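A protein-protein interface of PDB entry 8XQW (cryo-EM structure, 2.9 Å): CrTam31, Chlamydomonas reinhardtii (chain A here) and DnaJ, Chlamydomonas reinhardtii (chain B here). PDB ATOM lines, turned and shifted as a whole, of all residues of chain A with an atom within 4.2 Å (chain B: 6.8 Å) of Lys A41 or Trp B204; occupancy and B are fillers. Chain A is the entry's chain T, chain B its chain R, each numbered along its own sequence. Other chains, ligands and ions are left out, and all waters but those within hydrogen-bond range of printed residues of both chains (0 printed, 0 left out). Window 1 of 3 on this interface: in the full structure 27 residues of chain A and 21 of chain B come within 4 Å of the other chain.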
ATOM      1  N   SEP A  18      -7.757  18.495 -25.923  1.00  0.00           N
ATOM      2  CA  SEP A  18      -9.067  18.114 -25.403  1.00  0.00           C
ATOM      3  CB  SEP A  18      -9.100  16.612 -25.126  1.00  0.00           C
ATOM      4  OG  SEP A  18      -8.108  16.264 -24.179  1.00  0.00           O
ATOM      5  C   SEP A  18      -9.473  18.864 -24.136  1.00  0.00           C
ATOM      6  O   SEP A  18     -10.605  19.330 -24.025  1.00  0.00           O
ATOM      7  P   SEP A  18      -8.200  14.711 -23.774  1.00  0.00           P
ATOM      8  O1P SEP A  18      -7.096  14.400 -22.647  1.00  0.00           O
ATOM      9  O2P SEP A  18      -7.921  13.803 -25.073  1.00  0.00           O
ATOM     10  O3P SEP A  18      -9.659  14.388 -23.174  1.00  0.00           O
ATOM     11  N   LEU A  38      -1.393  15.378 -14.994  1.00  0.00           N
ATOM     12  CA  LEU A  38      -1.865  14.368 -14.056  1.00  0.00           C
ATOM     13  C   LEU A  38      -2.349  13.086 -14.723  1.00  0.00           C
ATOM     14  O   LEU A  38      -2.808  12.179 -14.020  1.00  0.00           O
ATOM     15  CB  LEU A  38      -2.981  14.943 -13.184  1.00  0.00           C
ATOM     16  CG  LEU A  38      -2.519  15.807 -12.016  1.00  0.00           C
ATOM     17  CD1 LEU A  38      -3.700  16.379 -11.277  1.00  0.00           C
ATOM     18  CD2 LEU A  38      -1.660  14.996 -11.081  1.00  0.00           C
ATOM     19  N   GLY A  39      -2.264  12.975 -16.045  1.00  0.00           N
ATOM     20  CA  GLY A  39      -2.738  11.792 -16.729  1.00  0.00           C
ATOM     21  C   GLY A  39      -3.519  12.135 -17.978  1.00  0.00           C
ATOM     22  O   GLY A  39      -4.070  13.231 -18.100  1.00  0.00           O
ATOM     23  N   PRO A  40      -3.567  11.209 -18.947  1.00  0.00           N
ATOM     24  CA  PRO A  40      -4.091  11.570 -20.272  1.00  0.00           C
ATOM     25  C   PRO A  40      -5.553  11.999 -20.276  1.00  0.00           C
ATOM     26  O   PRO A  40      -5.833  13.188 -20.462  1.00  0.00           O
ATOM     27  CB  PRO A  40      -3.897  10.280 -21.084  1.00  0.00           C
ATOM     28  CG  PRO A  40      -2.919   9.470 -20.304  1.00  0.00           C
ATOM     29  CD  PRO A  40      -3.170   9.797 -18.879  1.00  0.00           C
ATOM     30  N   LYS A  41      -6.499  11.078 -20.087  1.00  0.00           N
ATOM     31  CA  LYS A  41      -7.814  11.505 -19.626  1.00  0.00           C
ATOM     32  C   LYS A  41      -8.365  10.645 -18.499  1.00  0.00           C
ATOM     33  O   LYS A  41      -8.475  11.079 -17.350  1.00  0.00           O
ATOM     34  CB  LYS A  41      -8.787  11.502 -20.805  1.00  0.00           C
ATOM     35  CG  LYS A  41     -10.241  11.749 -20.439  1.00  0.00           C
ATOM     36  CD  LYS A  41     -11.100  11.778 -21.686  1.00  0.00           C
ATOM     37  CE  LYS A  41     -10.765  10.614 -22.603  1.00  0.00           C
ATOM     38  NZ  LYS A  41     -11.013   9.306 -21.939  1.00  0.00           N
ATOM     39  N   LYS A  42      -8.703   9.407 -18.846  1.00  0.00           N
ATOM     40  CA  LYS A  42      -9.221   8.416 -17.918  1.00  0.00           C
ATOM     41  C   LYS A  42      -9.137   7.060 -18.601  1.00  0.00           C
ATOM     42  O   LYS A  42      -9.995   6.731 -19.425  1.00  0.00           O
ATOM     43  CB  LYS A  42     -10.653   8.761 -17.515  1.00  0.00           C
ATOM     44  CG  LYS A  42     -11.214   7.938 -16.384  1.00  0.00           C
ATOM     45  CD  LYS A  42     -12.498   8.562 -15.877  1.00  0.00           C
ATOM     46  CE  LYS A  42     -13.085   7.786 -14.721  1.00  0.00           C
ATOM     47  NZ  LYS A  42     -14.053   8.605 -13.945  1.00  0.00           N
ATOM     48  N   ALA B 198     -12.691  21.182  -7.904  1.00  0.00           N
ATOM     49  CA  ALA B 198     -13.910  20.932  -8.660  1.00  0.00           C
ATOM     50  C   ALA B 198     -13.590  20.401 -10.049  1.00  0.00           C
ATOM     51  O   ALA B 198     -14.235  19.460 -10.524  1.00  0.00           O
ATOM     52  CB  ALA B 198     -14.736  22.211  -8.750  1.00  0.00           C
ATOM     53  N   ALA B 199     -12.596  20.989 -10.712  1.00  0.00           N
ATOM     54  CA  ALA B 199     -12.187  20.485 -12.020  1.00  0.00           C
ATOM     55  C   ALA B 199     -11.661  19.062 -11.912  1.00  0.00           C
ATOM     56  O   ALA B 199     -11.911  18.222 -12.786  1.00  0.00           O
ATOM     57  CB  ALA B 199     -11.130  21.406 -12.629  1.00  0.00           C
ATOM     58  N   LEU B 200     -10.921  18.777 -10.840  1.00  0.00           N
ATOM     59  CA  LEU B 200     -10.439  17.419 -10.607  1.00  0.00           C
ATOM     60  C   LEU B 200     -11.596  16.443 -10.460  1.00  0.00           C
ATOM     61  O   LEU B 200     -11.573  15.346 -11.029  1.00  0.00           O
ATOM     62  CB  LEU B 200      -9.556  17.382  -9.363  1.00  0.00           C
ATOM     63  CG  LEU B 200      -8.083  17.722  -9.548  1.00  0.00           C
ATOM     64  CD1 LEU B 200      -7.586  18.519  -8.369  1.00  0.00           C
ATOM     65  CD2 LEU B 200      -7.294  16.445  -9.683  1.00  0.00           C
ATOM     66  N   MET B 201     -12.618  16.824  -9.693  1.00  0.00           N
ATOM     67  CA  MET B 201     -13.791  15.973  -9.542  1.00  0.00           C
ATOM     68  C   MET B 201     -14.524  15.805 -10.866  1.00  0.00           C
ATOM     69  O   MET B 201     -15.129  14.759 -11.121  1.00  0.00           O
ATOM     70  CB  MET B 201     -14.727  16.558  -8.489  1.00  0.00           C
ATOM     71  CG  MET B 201     -15.623  15.535  -7.834  1.00  0.00           C
ATOM     72  SD  MET B 201     -14.937  14.930  -6.292  1.00  0.00           S
ATOM     73  CE  MET B 201     -15.860  13.414  -6.083  1.00  0.00           C
ATOM     74  N   ARG B 202     -14.490  16.832 -11.715  1.00  0.00           N
ATOM     75  CA  ARG B 202     -15.216  16.764 -12.978  1.00  0.00           C
ATOM     76  C   ARG B 202     -14.504  15.868 -13.981  1.00  0.00           C
ATOM     77  O   ARG B 202     -15.154  15.194 -14.789  1.00  0.00           O
ATOM     78  CB  ARG B 202     -15.408  18.166 -13.550  1.00  0.00           C
ATOM     79  CG  ARG B 202     -16.672  18.857 -13.061  1.00  0.00           C
ATOM     80  CD  ARG B 202     -16.761  20.292 -13.553  1.00  0.00           C
ATOM     81  NE  ARG B 202     -16.769  20.375 -15.008  1.00  0.00           N
ATOM     82  CZ  ARG B 202     -16.638  21.508 -15.690  1.00  0.00           C
ATOM     83  NH1 ARG B 202     -16.481  22.654 -15.043  1.00  0.00           N
ATOM     84  NH2 ARG B 202     -16.654  21.495 -17.013  1.00  0.00           N
ATOM     85  N   ARG B 203     -13.173  15.843 -13.950  1.00  0.00           N
ATOM     86  CA  ARG B 203     -12.448  14.989 -14.885  1.00  0.00           C
ATOM     87  C   ARG B 203     -12.451  13.535 -14.431  1.00  0.00           C
ATOM     88  O   ARG B 203     -12.968  12.663 -15.136  1.00  0.00           O
ATOM     89  CB  ARG B 203     -11.019  15.492 -15.054  1.00  0.00           C
ATOM     90  CG  ARG B 203     -10.284  14.902 -16.239  1.00  0.00           C
ATOM     91  CD  ARG B 203      -9.313  15.923 -16.781  1.00  0.00           C
ATOM     92  NE  ARG B 203      -8.393  15.395 -17.780  1.00  0.00           N
ATOM     93  CZ  ARG B 203      -8.725  15.101 -19.030  1.00  0.00           C
ATOM     94  NH1 ARG B 203      -9.970  15.268 -19.447  1.00  0.00           N
ATOM     95  NH2 ARG B 203      -7.809  14.642 -19.868  1.00  0.00           N
ATOM     96  N   TRP B 204     -11.882  13.258 -13.261  1.00  0.00           N
ATOM     97  CA  TRP B 204     -11.894  11.931 -12.663  1.00  0.00           C
ATOM     98  C   TRP B 204     -12.938  11.913 -11.563  1.00  0.00           C
ATOM     99  O   TRP B 204     -13.048  12.873 -10.794  1.00  0.00           O
ATOM    100  CB  TRP B 204     -10.524  11.560 -12.086  1.00  0.00           C
ATOM    101  CG  TRP B 204      -9.414  11.594 -13.072  1.00  0.00           C
ATOM    102  CD1 TRP B 204      -9.110  10.644 -13.995  1.00  0.00           C
ATOM    103  CD2 TRP B 204      -8.451  12.636 -13.239  1.00  0.00           C
ATOM    104  NE1 TRP B 204      -8.020  11.027 -14.728  1.00  0.00           N
ATOM    105  CE2 TRP B 204      -7.596  12.249 -14.282  1.00  0.00           C
ATOM    106  CE3 TRP B 204      -8.233  13.860 -12.609  1.00  0.00           C
ATOM    107  CZ2 TRP B 204      -6.542  13.041 -14.710  1.00  0.00           C
ATOM    108  CZ3 TRP B 204      -7.185  14.642 -13.032  1.00  0.00           C
ATOM    109  CH2 TRP B 204      -6.355  14.233 -14.074  1.00  0.00           C
ATOM    110  N   GLY B 205     -13.705  10.834 -11.488  1.00  0.00           N
ATOM    111  CA  GLY B 205     -14.709  10.729 -10.456  1.00  0.00           C
ATOM    112  C   GLY B 205     -14.083  10.475  -9.096  1.00  0.00           C
ATOM    113  O   GLY B 205     -12.870  10.534  -8.903  1.00  0.00           O
ATOM    114  N   HIS B 206     -14.947  10.205  -8.134  1.00  0.00           N
ATOM    115  CA  HIS B 206     -14.474   9.666  -6.875  1.00  0.00           C
ATOM    116  C   HIS B 206     -13.833   8.312  -7.149  1.00  0.00           C
ATOM    117  O   HIS B 206     -14.356   7.543  -7.965  1.00  0.00           O
ATOM    118  CB  HIS B 206     -15.622   9.522  -5.883  1.00  0.00           C
ATOM    119  CG  HIS B 206     -15.187   9.114  -4.513  1.00  0.00           C
ATOM    120  ND1 HIS B 206     -14.969   7.800  -4.164  1.00  0.00           N
ATOM    121  CD2 HIS B 206     -14.922   9.848  -3.405  1.00  0.00           C
ATOM    122  CE1 HIS B 206     -14.594   7.740  -2.899  1.00  0.00           C
ATOM    123  NE2 HIS B 206     -14.558   8.968  -2.416  1.00  0.00           N
ATOM    124  N   PRO B 207     -12.706   7.986  -6.511  1.00  0.00           N
ATOM    125  CA  PRO B 207     -11.974   6.765  -6.886  1.00  0.00           C
ATOM    126  C   PRO B 207     -12.797   5.494  -6.811  1.00  0.00           C
ATOM    127  O   PRO B 207     -12.526   4.559  -7.572  1.00  0.00           O
ATOM    128  CB  PRO B 207     -10.810   6.735  -5.889  1.00  0.00           C
ATOM    129  CG  PRO B 207     -11.213   7.656  -4.788  1.00  0.00           C
ATOM    130  CD  PRO B 207     -12.017   8.722  -5.442  1.00  0.00           C
ATOM    131  N   ALA B 210     -14.712   5.018 -10.357  1.00  0.00           N
ATOM    132  CA  ALA B 210     -13.881   4.616 -11.478  1.00  0.00           C
ATOM    133  C   ALA B 210     -13.198   3.279 -11.251  1.00  0.00           C
ATOM    134  O   ALA B 210     -12.430   2.838 -12.112  1.00  0.00           O
ATOM    135  CB  ALA B 210     -12.829   5.689 -11.758  1.00  0.00           C
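O1P of SEP A18 lies close to NH2 of Arg B203 (2.9 Å).
The backbone carbonyl oxygen (O) of Pro A40 is in hydrogen-bond range of the guanidinium group (NH2) of Arg B203, 2.5 Å away.
The indole nitrogen (NE1) of Trp B204 is in hydrogen-bond range of the backbone carbonyl oxygen (O) of Lys A41, 2.7 Å away.
NZ of Lys A42 lies close to N of Gly B205, 3.3 Å away.
O of Pro A40 sits close to O1P of SEP A18 (2.8 Å).
Among the printed residues, pairs that only touch across the chains: Lys A41 with Arg B203, Leu A38 with Trp B204, Lys A42 with Ala B210 and Leu A38 with Leu B200.
Of chain B, only Arg B203 and Trp B204 come within 4 Å of Lys A41.
Of the printed residues of chain B, Pro A40 touches Arg B203 (2.5 Å).
Of the printed residues of chain A, Leu B200 touches Leu A38.
Of the printed residues of chain B, SEP A18 touches Arg B203.
The nearest printed residue of chain A that does not touch Ala B210 is Lys A41 (8.9 Å).
Of the 11 printed residues of chain B, 5 touch a printed residue of chain A.
Along chain B the printed residues that touch a printed residue of chain A span positions 200 to 210.
Of the 6 printed residues of chain A, 5 touch a printed residue of chain B.
Hydrophobic or aromatic side chains of chain A within 4 Å of the printed part of chain B: Leu A38.
Among the printed residues, 8 pairs touch across the chains.
Among the printed residues, no Asp or Glu carboxylate lies within 4 Å of a Lys or Arg side-chain nitrogen of the other chain.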
